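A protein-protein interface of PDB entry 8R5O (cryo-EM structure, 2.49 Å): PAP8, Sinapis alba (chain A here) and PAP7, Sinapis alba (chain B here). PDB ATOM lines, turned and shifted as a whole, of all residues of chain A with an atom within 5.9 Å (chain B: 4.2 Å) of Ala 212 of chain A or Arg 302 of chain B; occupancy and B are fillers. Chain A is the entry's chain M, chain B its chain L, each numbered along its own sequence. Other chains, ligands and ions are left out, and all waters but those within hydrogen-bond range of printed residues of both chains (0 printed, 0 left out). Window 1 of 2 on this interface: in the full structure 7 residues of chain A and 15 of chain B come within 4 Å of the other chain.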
ATOM      1  N   ILE A 210      -3.584  19.396   3.436  1.00  0.00           N
ATOM      2  CA  ILE A 210      -4.110  18.323   2.601  1.00  0.00           C
ATOM      3  C   ILE A 210      -4.417  17.148   3.521  1.00  0.00           C
ATOM      4  O   ILE A 210      -3.533  16.357   3.857  1.00  0.00           O
ATOM      5  CB  ILE A 210      -3.128  17.948   1.490  1.00  0.00           C
ATOM      6  CG1 ILE A 210      -2.838  19.173   0.620  1.00  0.00           C
ATOM      7  CG2 ILE A 210      -3.673  16.806   0.647  1.00  0.00           C
ATOM      8  CD1 ILE A 210      -1.832  18.929  -0.472  1.00  0.00           C
ATOM      9  N   ASP A 211      -5.677  17.037   3.941  1.00  0.00           N
ATOM     10  CA  ASP A 211      -6.095  15.968   4.843  1.00  0.00           C
ATOM     11  C   ASP A 211      -6.611  14.753   4.075  1.00  0.00           C
ATOM     12  O   ASP A 211      -6.049  13.659   4.180  1.00  0.00           O
ATOM     13  CB  ASP A 211      -7.167  16.493   5.807  1.00  0.00           C
ATOM     14  CG  ASP A 211      -7.369  15.586   7.008  1.00  0.00           C
ATOM     15  OD1 ASP A 211      -6.735  14.512   7.063  1.00  0.00           O
ATOM     16  OD2 ASP A 211      -8.161  15.950   7.904  1.00  0.00           O
ATOM     17  N   ALA A 212      -7.670  14.935   3.301  1.00  0.00           N
ATOM     18  CA  ALA A 212      -8.285  13.865   2.535  1.00  0.00           C
ATOM     19  C   ALA A 212      -7.562  13.670   1.210  1.00  0.00           C
ATOM     20  O   ALA A 212      -6.847  14.561   0.745  1.00  0.00           O
ATOM     21  CB  ALA A 212      -9.759  14.180   2.288  1.00  0.00           C
ATOM     22  N   PRO A 213      -7.711  12.502   0.583  1.00  0.00           N
ATOM     23  CA  PRO A 213      -7.140  12.314  -0.755  1.00  0.00           C
ATOM     24  C   PRO A 213      -7.714  13.312  -1.750  1.00  0.00           C
ATOM     25  O   PRO A 213      -8.899  13.646  -1.711  1.00  0.00           O
ATOM     26  CB  PRO A 213      -7.536  10.876  -1.109  1.00  0.00           C
ATOM     27  CG  PRO A 213      -7.699  10.207   0.200  1.00  0.00           C
ATOM     28  CD  PRO A 213      -8.252  11.246   1.129  1.00  0.00           C
ATOM     29  N   ARG A 214      -6.848  13.789  -2.648  1.00  0.00           N
ATOM     30  CA  ARG A 214      -7.205  14.761  -3.684  1.00  0.00           C
ATOM     31  C   ARG A 214      -7.703  16.078  -3.094  1.00  0.00           C
ATOM     32  O   ARG A 214      -8.486  16.792  -3.724  1.00  0.00           O
ATOM     33  CB  ARG A 214      -8.242  14.188  -4.655  1.00  0.00           C
ATOM     34  CG  ARG A 214      -7.775  12.959  -5.410  1.00  0.00           C
ATOM     35  CD  ARG A 214      -8.931  12.289  -6.126  1.00  0.00           C
ATOM     36  NE  ARG A 214      -9.966  11.855  -5.198  1.00  0.00           N
ATOM     37  CZ  ARG A 214      -9.984  10.675  -4.594  1.00  0.00           C
ATOM     38  NH1 ARG A 214      -9.036   9.777  -4.806  1.00  0.00           N
ATOM     39  NH2 ARG A 214     -10.976  10.390  -3.757  1.00  0.00           N
ATOM     40  N   ASP A 215      -7.263  16.412  -1.885  1.00  0.00           N
ATOM     41  CA  ASP A 215      -7.563  17.724  -1.333  1.00  0.00           C
ATOM     42  C   ASP A 215      -6.893  18.799  -2.186  1.00  0.00           C
ATOM     43  O   ASP A 215      -5.758  18.612  -2.640  1.00  0.00           O
ATOM     44  CB  ASP A 215      -7.090  17.827   0.116  1.00  0.00           C
ATOM     45  CG  ASP A 215      -8.201  17.571   1.112  1.00  0.00           C
ATOM     46  OD1 ASP A 215      -9.351  17.349   0.682  1.00  0.00           O
ATOM     47  OD2 ASP A 215      -7.923  17.598   2.329  1.00  0.00           O
ATOM     48  N   PRO B 123     -14.843   9.613  -6.912  1.00  0.00           N
ATOM     49  CA  PRO B 123     -14.173  10.062  -5.686  1.00  0.00           C
ATOM     50  C   PRO B 123     -15.156  10.257  -4.542  1.00  0.00           C
ATOM     51  O   PRO B 123     -16.327  10.578  -4.744  1.00  0.00           O
ATOM     52  CB  PRO B 123     -13.525  11.387  -6.103  1.00  0.00           C
ATOM     53  CG  PRO B 123     -13.415  11.309  -7.586  1.00  0.00           C
ATOM     54  CD  PRO B 123     -14.608  10.530  -8.038  1.00  0.00           C
ATOM     55  N   HIS B 124     -14.652  10.057  -3.323  1.00  0.00           N
ATOM     56  CA  HIS B 124     -15.490  10.160  -2.132  1.00  0.00           C
ATOM     57  C   HIS B 124     -16.024  11.575  -1.939  1.00  0.00           C
ATOM     58  O   HIS B 124     -17.165  11.760  -1.503  1.00  0.00           O
ATOM     59  CB  HIS B 124     -14.698   9.713  -0.903  1.00  0.00           C
ATOM     60  CG  HIS B 124     -15.462   9.804   0.381  1.00  0.00           C
ATOM     61  ND1 HIS B 124     -16.672   9.174   0.575  1.00  0.00           N
ATOM     62  CD2 HIS B 124     -15.182  10.445   1.540  1.00  0.00           C
ATOM     63  CE1 HIS B 124     -17.107   9.428   1.795  1.00  0.00           C
ATOM     64  NE2 HIS B 124     -16.221  10.196   2.402  1.00  0.00           N
ATOM     65  N   ILE B 268     -12.898   4.299   6.078  1.00  0.00           N
ATOM     66  CA  ILE B 268     -12.333   5.610   5.793  1.00  0.00           C
ATOM     67  C   ILE B 268     -11.212   5.827   6.796  1.00  0.00           C
ATOM     68  O   ILE B 268     -11.463   5.952   8.001  1.00  0.00           O
ATOM     69  CB  ILE B 268     -13.384   6.724   5.871  1.00  0.00           C
ATOM     70  CG1 ILE B 268     -14.464   6.497   4.813  1.00  0.00           C
ATOM     71  CG2 ILE B 268     -12.735   8.081   5.686  1.00  0.00           C
ATOM     72  CD1 ILE B 268     -15.521   7.572   4.772  1.00  0.00           C
ATOM     73  N   TRP B 297     -15.858  -0.532  -2.706  1.00  0.00           N
ATOM     74  CA  TRP B 297     -15.206   0.606  -2.077  1.00  0.00           C
ATOM     75  C   TRP B 297     -13.701   0.371  -2.014  1.00  0.00           C
ATOM     76  O   TRP B 297     -13.247  -0.668  -1.530  1.00  0.00           O
ATOM     77  CB  TRP B 297     -15.775   0.832  -0.678  1.00  0.00           C
ATOM     78  CG  TRP B 297     -15.104   1.926   0.090  1.00  0.00           C
ATOM     79  CD1 TRP B 297     -14.231   1.781   1.124  1.00  0.00           C
ATOM     80  CD2 TRP B 297     -15.255   3.334  -0.114  1.00  0.00           C
ATOM     81  NE1 TRP B 297     -13.827   3.010   1.578  1.00  0.00           N
ATOM     82  CE2 TRP B 297     -14.441   3.981   0.834  1.00  0.00           C
ATOM     83  CE3 TRP B 297     -15.999   4.112  -1.007  1.00  0.00           C
ATOM     84  CZ2 TRP B 297     -14.348   5.368   0.917  1.00  0.00           C
ATOM     85  CZ3 TRP B 297     -15.906   5.488  -0.922  1.00  0.00           C
ATOM     86  CH2 TRP B 297     -15.087   6.103   0.032  1.00  0.00           C
ATOM     87  N   ARG B 298     -12.931   1.336  -2.516  1.00  0.00           N
ATOM     88  CA  ARG B 298     -11.478   1.270  -2.457  1.00  0.00           C
ATOM     89  C   ARG B 298     -11.004   2.167  -1.322  1.00  0.00           C
ATOM     90  O   ARG B 298     -10.912   3.389  -1.504  1.00  0.00           O
ATOM     91  CB  ARG B 298     -10.857   1.705  -3.788  1.00  0.00           C
ATOM     92  CG  ARG B 298      -9.517   1.059  -4.090  1.00  0.00           C
ATOM     93  CD  ARG B 298      -8.781   1.795  -5.193  1.00  0.00           C
ATOM     94  NE  ARG B 298      -9.496   1.764  -6.462  1.00  0.00           N
ATOM     95  CZ  ARG B 298      -9.385   2.688  -7.405  1.00  0.00           C
ATOM     96  NH1 ARG B 298      -8.630   3.760  -7.238  1.00  0.00           N
ATOM     97  NH2 ARG B 298     -10.052   2.534  -8.545  1.00  0.00           N
ATOM     98  N   PRO B 299     -10.703   1.623  -0.141  1.00  0.00           N
ATOM     99  CA  PRO B 299     -10.407   2.487   1.014  1.00  0.00           C
ATOM    100  C   PRO B 299      -9.175   3.359   0.851  1.00  0.00           C
ATOM    101  O   PRO B 299      -9.144   4.467   1.398  1.00  0.00           O
ATOM    102  CB  PRO B 299     -10.226   1.485   2.164  1.00  0.00           C
ATOM    103  CG  PRO B 299     -10.835   0.213   1.682  1.00  0.00           C
ATOM    104  CD  PRO B 299     -10.627   0.197   0.208  1.00  0.00           C
ATOM    105  N   LYS B 300      -8.156   2.892   0.125  1.00  0.00           N
ATOM    106  CA  LYS B 300      -6.858   3.558   0.162  1.00  0.00           C
ATOM    107  C   LYS B 300      -6.925   4.966  -0.418  1.00  0.00           C
ATOM    108  O   LYS B 300      -6.319   5.895   0.128  1.00  0.00           O
ATOM    109  CB  LYS B 300      -5.819   2.715  -0.574  1.00  0.00           C
ATOM    110  CG  LYS B 300      -4.386   3.077  -0.238  1.00  0.00           C
ATOM    111  CD  LYS B 300      -3.524   1.833  -0.080  1.00  0.00           C
ATOM    112  CE  LYS B 300      -4.063   0.933   1.019  1.00  0.00           C
ATOM    113  NZ  LYS B 300      -3.232  -0.290   1.203  1.00  0.00           N
ATOM    114  N   ASP B 301      -7.656   5.153  -1.513  1.00  0.00           N
ATOM    115  CA  ASP B 301      -7.812   6.471  -2.113  1.00  0.00           C
ATOM    116  C   ASP B 301      -9.239   6.995  -2.018  1.00  0.00           C
ATOM    117  O   ASP B 301      -9.544   8.034  -2.610  1.00  0.00           O
ATOM    118  CB  ASP B 301      -7.352   6.450  -3.571  1.00  0.00           C
ATOM    119  CG  ASP B 301      -7.961   5.313  -4.351  1.00  0.00           C
ATOM    120  OD1 ASP B 301      -8.712   4.521  -3.750  1.00  0.00           O
ATOM    121  OD2 ASP B 301      -7.690   5.211  -5.563  1.00  0.00           O
ATOM    122  N   ARG B 302     -10.109   6.308  -1.277  1.00  0.00           N
ATOM    123  CA  ARG B 302     -11.496   6.723  -1.065  1.00  0.00           C
ATOM    124  C   ARG B 302     -12.221   6.925  -2.397  1.00  0.00           C
ATOM    125  O   ARG B 302     -12.709   8.008  -2.720  1.00  0.00           O
ATOM    126  CB  ARG B 302     -11.563   7.986  -0.201  1.00  0.00           C
ATOM    127  CG  ARG B 302     -10.826   7.870   1.111  1.00  0.00           C
ATOM    128  CD  ARG B 302     -11.059   9.089   1.968  1.00  0.00           C
ATOM    129  NE  ARG B 302     -10.176   9.103   3.126  1.00  0.00           N
ATOM    130  CZ  ARG B 302     -10.166  10.054   4.047  1.00  0.00           C
ATOM    131  NH1 ARG B 302     -10.984  11.091   3.978  1.00  0.00           N
ATOM    132  NH2 ARG B 302      -9.317   9.960   5.065  1.00  0.00           N
ATOM    133  N   ILE B 303     -12.274   5.850  -3.174  1.00  0.00           N
ATOM    134  CA  ILE B 303     -12.936   5.845  -4.470  1.00  0.00           C
ATOM    135  C   ILE B 303     -13.909   4.677  -4.506  1.00  0.00           C
ATOM    136  O   ILE B 303     -13.546   3.552  -4.149  1.00  0.00           O
ATOM    137  CB  ILE B 303     -11.920   5.749  -5.625  1.00  0.00           C
ATOM    138  CG1 ILE B 303     -11.241   7.103  -5.838  1.00  0.00           C
ATOM    139  CG2 ILE B 303     -12.587   5.261  -6.903  1.00  0.00           C
ATOM    140  CD1 ILE B 303     -10.210   7.100  -6.930  1.00  0.00           C
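Ala 212 of chain A touches just one residue of chain B: Arg 302 (3.7 Å). Arg 302 of chain B touches just these residues of chain A: Ala 212, Pro 213 and Arg 214. Of the printed residues of chain B, Pro 213 of chain A touches Asp 301 and Arg 302. Of the printed residues of chain A, Asp 301 of chain B touches Pro 213 and Arg 214. Of the printed residues of chain A, Ile 303 of chain B touches Arg 214. Printed residues of chain A within 4 Å of His 124 of chain B: Arg 214.
The guanidinium group (NH1) of Arg 298 of chain B lies within salt-bridge range of the side-chain carboxylate (OD2) of Asp 301 of chain B (2.4 Å). The backbone carbonyl oxygen of Ile 303 of chain B is in hydrogen-bond range of the backbone NH of Arg 298 of chain B (2.8 Å). N of His 124 of chain B sits at hydrogen-bond distance from O of Arg 302 of chain B, at 2.9 Å. The backbone NH (N) of Ala 212 of chain A is in hydrogen-bond range of the side-chain carboxylate (OD2) of Asp 215 of chain A, at 2.8 Å.
The backbone carbonyl oxygen (O) of Asp 301 of chain B is in hydrogen-bond range of the guanidinium group (NH1) of Arg 214 of chain A. The backbone carbonyl oxygen (O) of Arg 302 of chain B is in hydrogen-bond range of the guanidinium group (NH2) of Arg 214 of chain A.
Among the printed residues, pairs that only touch across the chains: Pro 213 of chain A with Arg 302 of chain B (3.5 Å), Arg 214 of chain A with Pro 123 of chain B (3.6 Å), Arg 214 of chain A with Ile 303 of chain B (3.6 Å), Arg 214 of chain A with His 124 of chain B (3.7 Å), Ala 212 of chain A with Arg 302 of chain B (3.7 Å) and Pro 213 of chain A with Asp 301 of chain B (3.8 Å).
Printed residues of chain B that touch a printed residue of chain A: Pro 123, His 124, Asp 301, Arg 302 and Ile 303. Hydrophobic or aromatic side chains of chain B within 4 Å of the printed part of chain A: Pro 123 and Ile 303. Along chain B the printed residues that touch a printed residue of chain A span positions 123 to 303. Printed residues of chain A that touch a printed residue of chain B: Ala 212, Pro 213 and Arg 214. Among the printed residues, no Asp or Glu carboxylate lies within 4 Å of a Lys or Arg side-chain nitrogen of the other chain.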
